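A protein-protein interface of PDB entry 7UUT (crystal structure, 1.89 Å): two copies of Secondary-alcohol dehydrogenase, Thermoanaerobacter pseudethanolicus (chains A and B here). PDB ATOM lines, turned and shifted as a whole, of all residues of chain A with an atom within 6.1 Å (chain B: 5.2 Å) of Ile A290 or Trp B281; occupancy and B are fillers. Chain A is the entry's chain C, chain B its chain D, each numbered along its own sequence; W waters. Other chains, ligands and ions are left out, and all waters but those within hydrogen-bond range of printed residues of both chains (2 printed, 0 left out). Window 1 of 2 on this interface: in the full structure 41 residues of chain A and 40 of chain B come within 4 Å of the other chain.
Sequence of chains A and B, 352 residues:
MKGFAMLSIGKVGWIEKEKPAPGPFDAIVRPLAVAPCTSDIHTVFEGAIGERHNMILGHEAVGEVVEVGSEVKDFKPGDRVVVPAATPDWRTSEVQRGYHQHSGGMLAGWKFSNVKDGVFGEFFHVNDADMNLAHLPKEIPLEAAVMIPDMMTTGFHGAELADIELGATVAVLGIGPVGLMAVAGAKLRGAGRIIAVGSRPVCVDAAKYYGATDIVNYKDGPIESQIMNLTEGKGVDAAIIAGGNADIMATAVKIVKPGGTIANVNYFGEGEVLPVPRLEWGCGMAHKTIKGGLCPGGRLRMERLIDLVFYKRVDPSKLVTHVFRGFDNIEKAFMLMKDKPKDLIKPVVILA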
ATOM      1  N   MET A 106      -8.904  -5.035  -4.864  1.00  0.00           N
ATOM      2  CA  MET A 106     -10.126  -5.479  -4.207  1.00  0.00           C
ATOM      3  C   MET A 106      -9.812  -6.034  -2.825  1.00  0.00           C
ATOM      4  O   MET A 106      -8.972  -6.927  -2.678  1.00  0.00           O
ATOM      5  CB  MET A 106     -10.830  -6.535  -5.060  1.00  0.00           C
ATOM      6  CG  MET A 106     -12.261  -6.828  -4.631  1.00  0.00           C
ATOM      7  SD  MET A 106     -13.115  -7.871  -5.831  1.00  0.00           S
ATOM      8  CE  MET A 106     -12.003  -9.274  -5.923  1.00  0.00           C
ATOM      9  N   MET A 249     -29.090 -14.683  -0.570  1.00  0.00           N
ATOM     10  CA  MET A 249     -29.248 -13.575  -1.508  1.00  0.00           C
ATOM     11  C   MET A 249     -30.606 -13.629  -2.198  1.00  0.00           C
ATOM     12  O   MET A 249     -31.266 -12.597  -2.374  1.00  0.00           O
ATOM     13  CB  MET A 249     -28.120 -13.605  -2.539  1.00  0.00           C
ATOM     14  CG  MET A 249     -28.253 -12.567  -3.639  1.00  0.00           C
ATOM     15  SD  MET A 249     -28.152 -10.881  -3.009  1.00  0.00           S
ATOM     16  CE  MET A 249     -26.448 -10.819  -2.459  1.00  0.00           C
ATOM     17  N   VAL A 253     -33.723 -10.733  -1.878  1.00  0.00           N
ATOM     18  CA  VAL A 253     -34.403 -10.112  -3.012  1.00  0.00           C
ATOM     19  C   VAL A 253     -35.905 -10.346  -2.926  1.00  0.00           C
ATOM     20  O   VAL A 253     -36.706  -9.464  -3.259  1.00  0.00           O
ATOM     21  CB  VAL A 253     -33.817 -10.636  -4.337  1.00  0.00           C
ATOM     22  CG1 VAL A 253     -34.620 -10.124  -5.524  1.00  0.00           C
ATOM     23  CG2 VAL A 253     -32.363 -10.222  -4.469  1.00  0.00           C
ATOM     24  N   GLY A 260     -36.455  -0.975  -3.080  1.00  0.00           N
ATOM     25  CA  GLY A 260     -35.703  -1.109  -1.853  1.00  0.00           C
ATOM     26  C   GLY A 260     -34.260  -1.486  -2.118  1.00  0.00           C
ATOM     27  O   GLY A 260     -33.786  -1.514  -3.255  1.00  0.00           O
ATOM     28  N   THR A 261     -33.550  -1.793  -1.036  1.00  0.00           N
ATOM     29  CA  THR A 261     -32.121  -2.056  -1.105  1.00  0.00           C
ATOM     30  C   THR A 261     -31.774  -3.347  -0.380  1.00  0.00           C
ATOM     31  O   THR A 261     -32.261  -3.604   0.722  1.00  0.00           O
ATOM     32  CB  THR A 261     -31.319  -0.896  -0.500  1.00  0.00           C
ATOM     33  OG1 THR A 261     -31.681   0.323  -1.157  1.00  0.00           O
ATOM     34  CG2 THR A 261     -29.824  -1.125  -0.683  1.00  0.00           C
ATOM     35  N   ILE A 262     -30.927  -4.157  -1.009  1.00  0.00           N
ATOM     36  CA  ILE A 262     -30.297  -5.300  -0.363  1.00  0.00           C
ATOM     37  C   ILE A 262     -28.871  -4.885  -0.044  1.00  0.00           C
ATOM     38  O   ILE A 262     -28.079  -4.615  -0.954  1.00  0.00           O
ATOM     39  CB  ILE A 262     -30.312  -6.550  -1.255  1.00  0.00           C
ATOM     40  CG1 ILE A 262     -31.738  -7.053  -1.480  1.00  0.00           C
ATOM     41  CG2 ILE A 262     -29.464  -7.651  -0.623  1.00  0.00           C
ATOM     42  CD1 ILE A 262     -32.408  -6.475  -2.698  1.00  0.00           C
ATOM     43  N   ALA A 263     -28.548  -4.810   1.241  1.00  0.00           N
ATOM     44  CA  ALA A 263     -27.220  -4.425   1.701  1.00  0.00           C
ATOM     45  C   ALA A 263     -26.536  -5.653   2.283  1.00  0.00           C
ATOM     46  O   ALA A 263     -26.958  -6.168   3.322  1.00  0.00           O
ATOM     47  CB  ALA A 263     -27.312  -3.309   2.738  1.00  0.00           C
ATOM     48  N   ASN A 264     -25.462  -6.101   1.640  1.00  0.00           N
ATOM     49  CA  ASN A 264     -24.727  -7.275   2.084  1.00  0.00           C
ATOM     50  C   ASN A 264     -23.419  -6.864   2.741  1.00  0.00           C
ATOM     51  O   ASN A 264     -22.664  -6.059   2.186  1.00  0.00           O
ATOM     52  CB  ASN A 264     -24.425  -8.230   0.930  1.00  0.00           C
ATOM     53  CG  ASN A 264     -23.474  -9.338   1.342  1.00  0.00           C
ATOM     54  OD1 ASN A 264     -23.836 -10.228   2.113  1.00  0.00           O
ATOM     55  ND2 ASN A 264     -22.243  -9.279   0.847  1.00  0.00           N
ATOM     56  N   PHE A 268     -19.162 -14.348   2.031  1.00  0.00           N
ATOM     57  CA  PHE A 268     -19.488 -15.657   1.476  1.00  0.00           C
ATOM     58  C   PHE A 268     -18.208 -16.445   1.225  1.00  0.00           C
ATOM     59  O   PHE A 268     -17.371 -16.040   0.410  1.00  0.00           O
ATOM     60  CB  PHE A 268     -20.290 -15.509   0.185  1.00  0.00           C
ATOM     61  CG  PHE A 268     -21.627 -14.849   0.374  1.00  0.00           C
ATOM     62  CD1 PHE A 268     -22.746 -15.599   0.701  1.00  0.00           C
ATOM     63  CD2 PHE A 268     -21.765 -13.480   0.225  1.00  0.00           C
ATOM     64  CE1 PHE A 268     -23.980 -14.995   0.879  1.00  0.00           C
ATOM     65  CE2 PHE A 268     -22.997 -12.867   0.401  1.00  0.00           C
ATOM     66  CZ  PHE A 268     -24.104 -13.627   0.727  1.00  0.00           C
ATOM     67  N   LEU A 274     -23.420 -16.259  -6.498  1.00  0.00           N
ATOM     68  CA  LEU A 274     -24.489 -15.858  -5.597  1.00  0.00           C
ATOM     69  C   LEU A 274     -25.757 -15.662  -6.409  1.00  0.00           C
ATOM     70  O   LEU A 274     -25.799 -14.760  -7.262  1.00  0.00           O
ATOM     71  CB  LEU A 274     -24.128 -14.570  -4.866  1.00  0.00           C
ATOM     72  CG  LEU A 274     -22.799 -14.530  -4.109  1.00  0.00           C
ATOM     73  CD1 LEU A 274     -22.632 -13.192  -3.410  1.00  0.00           C
ATOM     74  CD2 LEU A 274     -22.685 -15.680  -3.116  1.00  0.00           C
ATOM     75  N   VAL A 276     -29.242 -14.519  -7.892  1.00  0.00           N
ATOM     76  CA  VAL A 276     -30.240 -13.459  -7.858  1.00  0.00           C
ATOM     77  C   VAL A 276     -31.460 -13.960  -8.629  1.00  0.00           C
ATOM     78  O   VAL A 276     -31.370 -14.186  -9.846  1.00  0.00           O
ATOM     79  CB  VAL A 276     -29.707 -12.148  -8.452  1.00  0.00           C
ATOM     80  CG1 VAL A 276     -30.823 -11.121  -8.563  1.00  0.00           C
ATOM     81  CG2 VAL A 276     -28.574 -11.601  -7.602  1.00  0.00           C
ATOM     82  N   TRP A 281     -36.504 -10.345  -8.907  1.00  0.00           N
ATOM     83  CA  TRP A 281     -35.753  -9.128  -9.186  1.00  0.00           C
ATOM     84  C   TRP A 281     -36.376  -8.322 -10.323  1.00  0.00           C
ATOM     85  O   TRP A 281     -35.691  -7.496 -10.940  1.00  0.00           O
ATOM     86  CB  TRP A 281     -34.292  -9.466  -9.509  1.00  0.00           C
ATOM     87  CG  TRP A 281     -33.319  -8.348  -9.235  1.00  0.00           C
ATOM     88  CD1 TRP A 281     -33.189  -7.640  -8.077  1.00  0.00           C
ATOM     89  CD2 TRP A 281     -32.341  -7.816 -10.141  1.00  0.00           C
ATOM     90  NE1 TRP A 281     -32.191  -6.700  -8.203  1.00  0.00           N
ATOM     91  CE2 TRP A 281     -31.656  -6.787  -9.460  1.00  0.00           C
ATOM     92  CE3 TRP A 281     -31.977  -8.111 -11.459  1.00  0.00           C
ATOM     93  CZ2 TRP A 281     -30.633  -6.049 -10.054  1.00  0.00           C
ATOM     94  CZ3 TRP A 281     -30.958  -7.376 -12.048  1.00  0.00           C
ATOM     95  CH2 TRP A 281     -30.299  -6.357 -11.344  1.00  0.00           C
ATOM     96  N   LYS A 288     -34.474  -3.071  -7.347  1.00  0.00           N
ATOM     97  CA  LYS A 288     -33.993  -3.631  -6.088  1.00  0.00           C
ATOM     98  C   LYS A 288     -32.471  -3.567  -6.119  1.00  0.00           C
ATOM     99  O   LYS A 288     -31.807  -4.437  -6.687  1.00  0.00           O
ATOM    100  CB  LYS A 288     -34.518  -5.047  -5.884  1.00  0.00           C
ATOM    101  CG  LYS A 288     -36.036  -5.099  -5.740  1.00  0.00           C
ATOM    102  CD  LYS A 288     -36.523  -6.489  -5.365  1.00  0.00           C
ATOM    103  CE  LYS A 288     -38.036  -6.573  -5.429  1.00  0.00           C
ATOM    104  NZ  LYS A 288     -38.523  -7.925  -5.039  1.00  0.00           N
ATOM    105  N   THR A 289     -31.923  -2.518  -5.513  1.00  0.00           N
ATOM    106  CA  THR A 289     -30.485  -2.309  -5.518  1.00  0.00           C
ATOM    107  C   THR A 289     -29.795  -3.318  -4.610  1.00  0.00           C
ATOM    108  O   THR A 289     -30.237  -3.579  -3.489  1.00  0.00           O
ATOM    109  CB  THR A 289     -30.163  -0.885  -5.067  1.00  0.00           C
ATOM    110  OG1 THR A 289     -30.775   0.046  -5.967  1.00  0.00           O
ATOM    111  CG2 THR A 289     -28.667  -0.644  -5.055  1.00  0.00           C
ATOM    112  N   ILE A 290     -28.706  -3.894  -5.105  1.00  0.00           N
ATOM    113  CA  ILE A 290     -27.910  -4.853  -4.354  1.00  0.00           C
ATOM    114  C   ILE A 290     -26.546  -4.231  -4.107  1.00  0.00           C
ATOM    115  O   ILE A 290     -25.827  -3.892  -5.055  1.00  0.00           O
ATOM    116  CB  ILE A 290     -27.786  -6.193  -5.091  1.00  0.00           C
ATOM    117  CG1 ILE A 290     -29.178  -6.736  -5.418  1.00  0.00           C
ATOM    118  CG2 ILE A 290     -26.999  -7.185  -4.246  1.00  0.00           C
ATOM    119  CD1 ILE A 290     -29.167  -7.960  -6.294  1.00  0.00           C
ATOM    120  N   LYS A 291     -26.203  -4.067  -2.835  1.00  0.00           N
ATOM    121  CA  LYS A 291     -24.909  -3.553  -2.420  1.00  0.00           C
ATOM    122  C   LYS A 291     -24.176  -4.603  -1.600  1.00  0.00           C
ATOM    123  O   LYS A 291     -24.791  -5.423  -0.912  1.00  0.00           O
ATOM    124  CB  LYS A 291     -25.060  -2.275  -1.594  1.00  0.00           C
ATOM    125  CG  LYS A 291     -25.724  -1.133  -2.332  1.00  0.00           C
ATOM    126  CD  LYS A 291     -25.806   0.069  -1.425  1.00  0.00           C
ATOM    127  CE  LYS A 291     -26.533   1.220  -2.075  1.00  0.00           C
ATOM    128  NZ  LYS A 291     -26.672   2.339  -1.104  1.00  0.00           N
ATOM    129  N   GLY A 292     -22.854  -4.583  -1.686  1.00  0.00           N
ATOM    130  CA  GLY A 292     -22.049  -5.464  -0.870  1.00  0.00           C
ATOM    131  C   GLY A 292     -20.676  -4.878  -0.643  1.00  0.00           C
ATOM    132  O   GLY A 292     -19.911  -4.743  -1.600  1.00  0.00           O
ATOM    133  N   VAL B 253     -19.952  -7.864 -13.564  1.00  0.00           N
ATOM    134  CA  VAL B 253     -19.287  -7.819 -12.264  1.00  0.00           C
ATOM    135  C   VAL B 253     -17.780  -7.950 -12.429  1.00  0.00           C
ATOM    136  O   VAL B 253     -17.003  -7.297 -11.722  1.00  0.00           O
ATOM    137  CB  VAL B 253     -19.858  -8.909 -11.337  1.00  0.00           C
ATOM    138  CG1 VAL B 253     -19.054  -8.996 -10.051  1.00  0.00           C
ATOM    139  CG2 VAL B 253     -21.314  -8.606 -11.017  1.00  0.00           C
ATOM    140  N   VAL B 276     -24.255 -13.939  -9.941  1.00  0.00           N
ATOM    141  CA  VAL B 276     -23.292 -12.955  -9.462  1.00  0.00           C
ATOM    142  C   VAL B 276     -22.061 -13.726  -8.991  1.00  0.00           C
ATOM    143  O   VAL B 276     -22.141 -14.478  -8.009  1.00  0.00           O
ATOM    144  CB  VAL B 276     -23.873 -12.087  -8.339  1.00  0.00           C
ATOM    145  CG1 VAL B 276     -22.802 -11.185  -7.744  1.00  0.00           C
ATOM    146  CG2 VAL B 276     -25.031 -11.257  -8.856  1.00  0.00           C
ATOM    147  N   PRO B 277     -20.913 -13.587  -9.656  1.00  0.00           N
ATOM    148  CA  PRO B 277     -19.737 -14.385  -9.279  1.00  0.00           C
ATOM    149  C   PRO B 277     -19.226 -13.981  -7.905  1.00  0.00           C
ATOM    150  O   PRO B 277     -18.992 -12.801  -7.640  1.00  0.00           O
ATOM    151  CB  PRO B 277     -18.720 -14.062 -10.379  1.00  0.00           C
ATOM    152  CG  PRO B 277     -19.126 -12.703 -10.864  1.00  0.00           C
ATOM    153  CD  PRO B 277     -20.625 -12.655 -10.760  1.00  0.00           C
ATOM    154  N   ARG B 278     -19.046 -14.975  -7.031  1.00  0.00           N
ATOM    155  CA  ARG B 278     -18.669 -14.686  -5.650  1.00  0.00           C
ATOM    156  C   ARG B 278     -17.298 -14.026  -5.573  1.00  0.00           C
ATOM    157  O   ARG B 278     -17.153 -12.944  -4.994  1.00  0.00           O
ATOM    158  CB  ARG B 278     -18.697 -15.966  -4.816  1.00  0.00           C
ATOM    159  CG  ARG B 278     -18.319 -15.753  -3.357  1.00  0.00           C
ATOM    160  CD  ARG B 278     -18.284 -17.064  -2.594  1.00  0.00           C
ATOM    161  NE  ARG B 278     -17.300 -17.994  -3.134  1.00  0.00           N
ATOM    162  CZ  ARG B 278     -16.044 -18.092  -2.714  1.00  0.00           C
ATOM    163  NH1 ARG B 278     -15.579 -17.329  -1.739  1.00  0.00           N
ATOM    164  NH2 ARG B 278     -15.238 -18.984  -3.284  1.00  0.00           N
ATOM    165  N   LEU B 279     -16.280 -14.656  -6.167  1.00  0.00           N
ATOM    166  CA  LEU B 279     -14.918 -14.140  -6.041  1.00  0.00           C
ATOM    167  C   LEU B 279     -14.792 -12.757  -6.669  1.00  0.00           C
ATOM    168  O   LEU B 279     -14.208 -11.844  -6.073  1.00  0.00           O
ATOM    169  CB  LEU B 279     -13.924 -15.113  -6.676  1.00  0.00           C
ATOM    170  CG  LEU B 279     -13.742 -16.449  -5.952  1.00  0.00           C
ATOM    171  CD1 LEU B 279     -12.777 -17.352  -6.711  1.00  0.00           C
ATOM    172  CD2 LEU B 279     -13.265 -16.221  -4.526  1.00  0.00           C
ATOM    173  N   GLU B 280     -15.340 -12.578  -7.874  1.00  0.00           N
ATOM    174  CA  GLU B 280     -15.242 -11.288  -8.548  1.00  0.00           C
ATOM    175  C   GLU B 280     -16.131 -10.224  -7.915  1.00  0.00           C
ATOM    176  O   GLU B 280     -15.928  -9.033  -8.175  1.00  0.00           O
ATOM    177  CB  GLU B 280     -15.579 -11.438 -10.033  1.00  0.00           C
ATOM    178  CG  GLU B 280     -14.482 -12.116 -10.857  1.00  0.00           C
ATOM    179  CD  GLU B 280     -14.552 -13.632 -10.814  1.00  0.00           C
ATOM    180  OE1 GLU B 280     -15.357 -14.176 -10.028  1.00  0.00           O
ATOM    181  OE2 GLU B 280     -13.804 -14.281 -11.577  1.00  0.00           O
ATOM    182  N   TRP B 281     -17.119 -10.617  -7.110  1.00  0.00           N
ATOM    183  CA  TRP B 281     -17.894  -9.663  -6.330  1.00  0.00           C
ATOM    184  C   TRP B 281     -17.272  -9.415  -4.961  1.00  0.00           C
ATOM    185  O   TRP B 281     -17.960  -8.935  -4.051  1.00  0.00           O
ATOM    186  CB  TRP B 281     -19.343 -10.141  -6.186  1.00  0.00           C
ATOM    187  CG  TRP B 281     -20.340  -9.034  -5.978  1.00  0.00           C
ATOM    188  CD1 TRP B 281     -20.484  -7.909  -6.736  1.00  0.00           C
ATOM    189  CD2 TRP B 281     -21.347  -8.960  -4.958  1.00  0.00           C
ATOM    190  NE1 TRP B 281     -21.509  -7.133  -6.245  1.00  0.00           N
ATOM    191  CE2 TRP B 281     -22.055  -7.757  -5.155  1.00  0.00           C
ATOM    192  CE3 TRP B 281     -21.716  -9.794  -3.898  1.00  0.00           C
ATOM    193  CZ2 TRP B 281     -23.109  -7.363  -4.328  1.00  0.00           C
ATOM    194  CZ3 TRP B 281     -22.762  -9.402  -3.076  1.00  0.00           C
ATOM    195  CH2 TRP B 281     -23.445  -8.198  -3.297  1.00  0.00           C
ATOM    196  N   GLY B 282     -15.984  -9.718  -4.804  1.00  0.00           N
ATOM    197  CA  GLY B 282     -15.302  -9.541  -3.536  1.00  0.00           C
ATOM    198  C   GLY B 282     -15.795 -10.448  -2.437  1.00  0.00           C
ATOM    199  O   GLY B 282     -15.711 -10.082  -1.259  1.00  0.00           O
ATOM    200  N   CYS B 283     -16.311 -11.629  -2.793  1.00  0.00           N
ATOM    201  CA  CYS B 283     -16.955 -12.537  -1.842  1.00  0.00           C
ATOM    202  C   CYS B 283     -18.087 -11.835  -1.095  1.00  0.00           C
ATOM    203  O   CYS B 283     -18.416 -12.192   0.040  1.00  0.00           O
ATOM    204  CB  CYS B 283     -15.942 -13.134  -0.859  1.00  0.00           C
ATOM    205  SG  CYS B 283     -14.517 -13.915  -1.654  1.00  0.00           S
ATOM    206  N   GLY B 284     -18.684 -10.836  -1.741  1.00  0.00           N
ATOM    207  CA  GLY B 284     -19.741 -10.037  -1.161  1.00  0.00           C
ATOM    208  C   GLY B 284     -19.332  -8.674  -0.643  1.00  0.00           C
ATOM    209  O   GLY B 284     -20.183  -7.963  -0.096  1.00  0.00           O
ATOM    210  N   MET B 285     -18.073  -8.262  -0.840  1.00  0.00           N
ATOM    211  CA  MET B 285     -17.542  -7.076  -0.177  1.00  0.00           C
ATOM    212  C   MET B 285     -16.785  -6.154  -1.127  1.00  0.00           C
ATOM    213  O   MET B 285     -15.991  -5.329  -0.667  1.00  0.00           O
ATOM    214  CB  MET B 285     -16.627  -7.482   0.984  1.00  0.00           C
ATOM    215  CG  MET B 285     -17.303  -8.349   2.045  1.00  0.00           C
ATOM    216  SD  MET B 285     -16.174  -8.976   3.302  1.00  0.00           S
ATOM    217  CE  MET B 285     -14.990  -9.851   2.280  1.00  0.00           C
ATOM    218  N   ALA B 286     -17.023  -6.255  -2.435  1.00  0.00           N
ATOM    219  CA  ALA B 286     -16.282  -5.470  -3.414  1.00  0.00           C
ATOM    220  C   ALA B 286     -16.884  -4.097  -3.672  1.00  0.00           C
ATOM    221  O   ALA B 286     -16.372  -3.368  -4.529  1.00  0.00           O
ATOM    222  CB  ALA B 286     -16.186  -6.232  -4.738  1.00  0.00           C
ATOM    223  N   LYS B 288     -19.351  -3.447  -5.317  1.00  0.00           N
ATOM    224  CA  LYS B 288     -19.850  -3.412  -6.688  1.00  0.00           C
ATOM    225  C   LYS B 288     -21.369  -3.391  -6.615  1.00  0.00           C
ATOM    226  O   LYS B 288     -22.013  -4.434  -6.491  1.00  0.00           O
ATOM    227  CB  LYS B 288     -19.330  -4.596  -7.494  1.00  0.00           C
ATOM    228  CG  LYS B 288     -17.822  -4.590  -7.679  1.00  0.00           C
ATOM    229  CD  LYS B 288     -17.369  -5.693  -8.622  1.00  0.00           C
ATOM    230  CE  LYS B 288     -15.853  -5.814  -8.635  1.00  0.00           C
ATOM    231  NZ  LYS B 288     -15.377  -6.879  -9.568  1.00  0.00           N
ATOM    232  N   THR B 289     -21.939  -2.191  -6.683  1.00  0.00           N
ATOM    233  CA  THR B 289     -23.383  -2.024  -6.585  1.00  0.00           C
ATOM    234  C   THR B 289     -24.050  -2.521  -7.858  1.00  0.00           C
ATOM    235  O   THR B 289     -23.603  -2.211  -8.966  1.00  0.00           O
ATOM    236  CB  THR B 289     -23.723  -0.550  -6.346  1.00  0.00           C
ATOM    237  OG1 THR B 289     -23.128  -0.116  -5.117  1.00  0.00           O
ATOM    238  CG2 THR B 289     -25.228  -0.333  -6.283  1.00  0.00           C
ATOM    239  N   ILE B 290     -25.128  -3.283  -7.703  1.00  0.00           N
ATOM    240  CA  ILE B 290     -25.891  -3.810  -8.828  1.00  0.00           C
ATOM    241  C   ILE B 290     -27.265  -3.159  -8.803  1.00  0.00           C
ATOM    242  O   ILE B 290     -28.020  -3.321  -7.837  1.00  0.00           O
ATOM    243  CB  ILE B 290     -26.011  -5.339  -8.768  1.00  0.00           C
ATOM    244  CG1 ILE B 290     -24.629  -5.976  -8.647  1.00  0.00           C
ATOM    245  CG2 ILE B 290     -26.733  -5.852 -10.008  1.00  0.00           C
ATOM    246  CD1 ILE B 290     -24.662  -7.474  -8.396  1.00  0.00           C
ATOM    247  N   LYS B 291     -27.592  -2.429  -9.863  1.00  0.00           N
ATOM    248  CA  LYS B 291     -28.900  -1.810 -10.005  1.00  0.00           C
ATOM    249  C   LYS B 291     -29.608  -2.371 -11.228  1.00  0.00           C
ATOM    250  O   LYS B 291     -28.974  -2.753 -12.220  1.00  0.00           O
ATOM    251  CB  LYS B 291     -28.797  -0.290 -10.128  1.00  0.00           C
ATOM    252  CG  LYS B 291     -28.174   0.408  -8.938  1.00  0.00           C
ATOM    253  CD  LYS B 291     -28.152   1.901  -9.196  1.00  0.00           C
ATOM    254  CE  LYS B 291     -27.465   2.676  -8.091  1.00  0.00           C
ATOM    255  NZ  LYS B 291     -27.374   4.124  -8.452  1.00  0.00           N
HETATM  256  O   HOH W   1     -21.913  -1.867  -2.895  1.00  0.00           O
HETATM  257  O   HOH W   2     -19.512  -6.092  -3.893  1.00  0.00           O
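The side-chain sulfur (SD) of Met A106 sits at hydrogen-bond distance from the backbone NH (N) of Gly B282.
O of Val B276 lies within hydrogen-bond range of N of Leu A274, 2.7 Å away.
The backbone carbonyl oxygen of Gly A292 sits at hydrogen-bond distance from the backbone NH of Ala B286.
O of Gly B284 sits at hydrogen-bond distance from ND2 of Asn A264, at 2.6 Å.
The backbone carbonyl oxygen (O) of Ile A290 is in hydrogen-bond range of the backbone NH (N) of Ile B290, 2.8 Å away.
The backbone carbonyl oxygen of Phe A268 is in hydrogen-bond range of the guanidinium group of Arg B278 (3.1 Å).
The backbone NH (N) of Phe A268 is in hydrogen-bond range of the backbone carbonyl oxygen (O) of Cys B283 (3.0 Å).
The backbone carbonyl oxygen of Gly A260 sits at hydrogen-bond distance from the backbone NH of Thr A289 (3.1 Å).
The backbone NH (N) of Ile A262 is in hydrogen-bond range of the backbone carbonyl oxygen (O) of Thr A289 (2.6 Å).
The backbone NH of Asn A264 is in hydrogen-bond range of the backbone carbonyl oxygen of Lys A291, at 2.7 Å.
NZ of Lys B288 lies within hydrogen-bond range of O of Val B253, at 2.7 Å.
The indole nitrogen (NE1) of Trp A281 sits at hydrogen-bond distance from the backbone carbonyl oxygen (O) of Lys A288.
The indole nitrogen of Trp B281 lies within hydrogen-bond range of the backbone carbonyl oxygen of Lys B288.
Met A106 touches Glu B280 (SD to O, 3.8 Å).
Met A106 touches Ala B286.
ND2 of Asn A264 touches CZ3 of Trp B281, 3.96 Å away.
Leu A274 touches Trp B281 (CD1 to CE3, 3.6 Å).
Trp A281 touches Lys B291.
OG1 of Thr A289 touches CG of Lys B291 (3.97 Å).
Thr B289 touches Ile A290 (CA to O, 3.4 Å).
Thr B289 touches Lys A291 (OG1 to CG, 3.9 Å).
Gly A292 touches Trp B281 (N to CZ2, 3.8 Å).
Gly B284 touches Gly A292 (O to C, 3.2 Å).
Ile A290 touches just these residues of chain B: Trp B281, Thr B289 and Ile B290.
Of the printed residues of chain B, Lys A291 touches Trp B281 (3.9 Å) and Thr B289 (3.9 Å).
Printed residues of chain B within 4 Å of Leu A274: Val B276 and Trp B281.
Ile A262 touches none of the printed residues of chain B.
The nearest residue of chain B that does not touch Ile A290 is Lys B288 (4.1 Å).
The nearest printed residue of chain A that does not touch Trp B281 is Met A106 (4.5 Å).
The nearest printed residue of chain B that does not touch Lys A291 is Ile B290 (5.0 Å).
Printed residues of chain B that touch a printed residue of chain A: Val B276, Arg B278, Leu B279, Glu B280, Trp B281, Gly B282, Cys B283, Gly B284, Met B285, Ala B286, Lys B288, Thr B289, Ile B290 and Lys B291.
Of the 17 printed residues of chain A, 11 touch a printed residue of chain B.
Hydrophobic or aromatic side chains of chain A within 4 Å of the printed part of chain B: Met A106, Met A249, Phe A268, Leu A274, Val A276, Trp A281 and Ile A290.
Among the printed residues, 27 pairs touch across the chains.
Among the printed residues, no Asp or Glu carboxylate lies within 4 Å of a Lys or Arg side-chain nitrogen of the other chain.
Trp A281 touches Ile B290, and with the chains exchanged Ile A290 touches Trp B281.
Thr A289 touches its own counterpart, Thr B289.
Thr A289 touches Ile B290, and with the chains exchanged Ile A290 touches Thr B289.
Ile A290 touches its own counterpart, Ile B290.
Positions printed for both chains: 253, 276, 281, 288, 289, 290 and 291.
Of the 27 pairs that touch across the chains among the printed residues, 11 have their exchanged pair printed and touching as well.
Water W2 lies within hydrogen-bond range of the backbone carbonyl oxygen (O) of Gly A292, the backbone NH (N) of Ala B286, the backbone NH (N) of Lys B288 and the backbone carbonyl oxygen (O) of Trp B281.
Water W1 lies within hydrogen-bond range of OG1 of Thr B289 and N of Gly A292.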
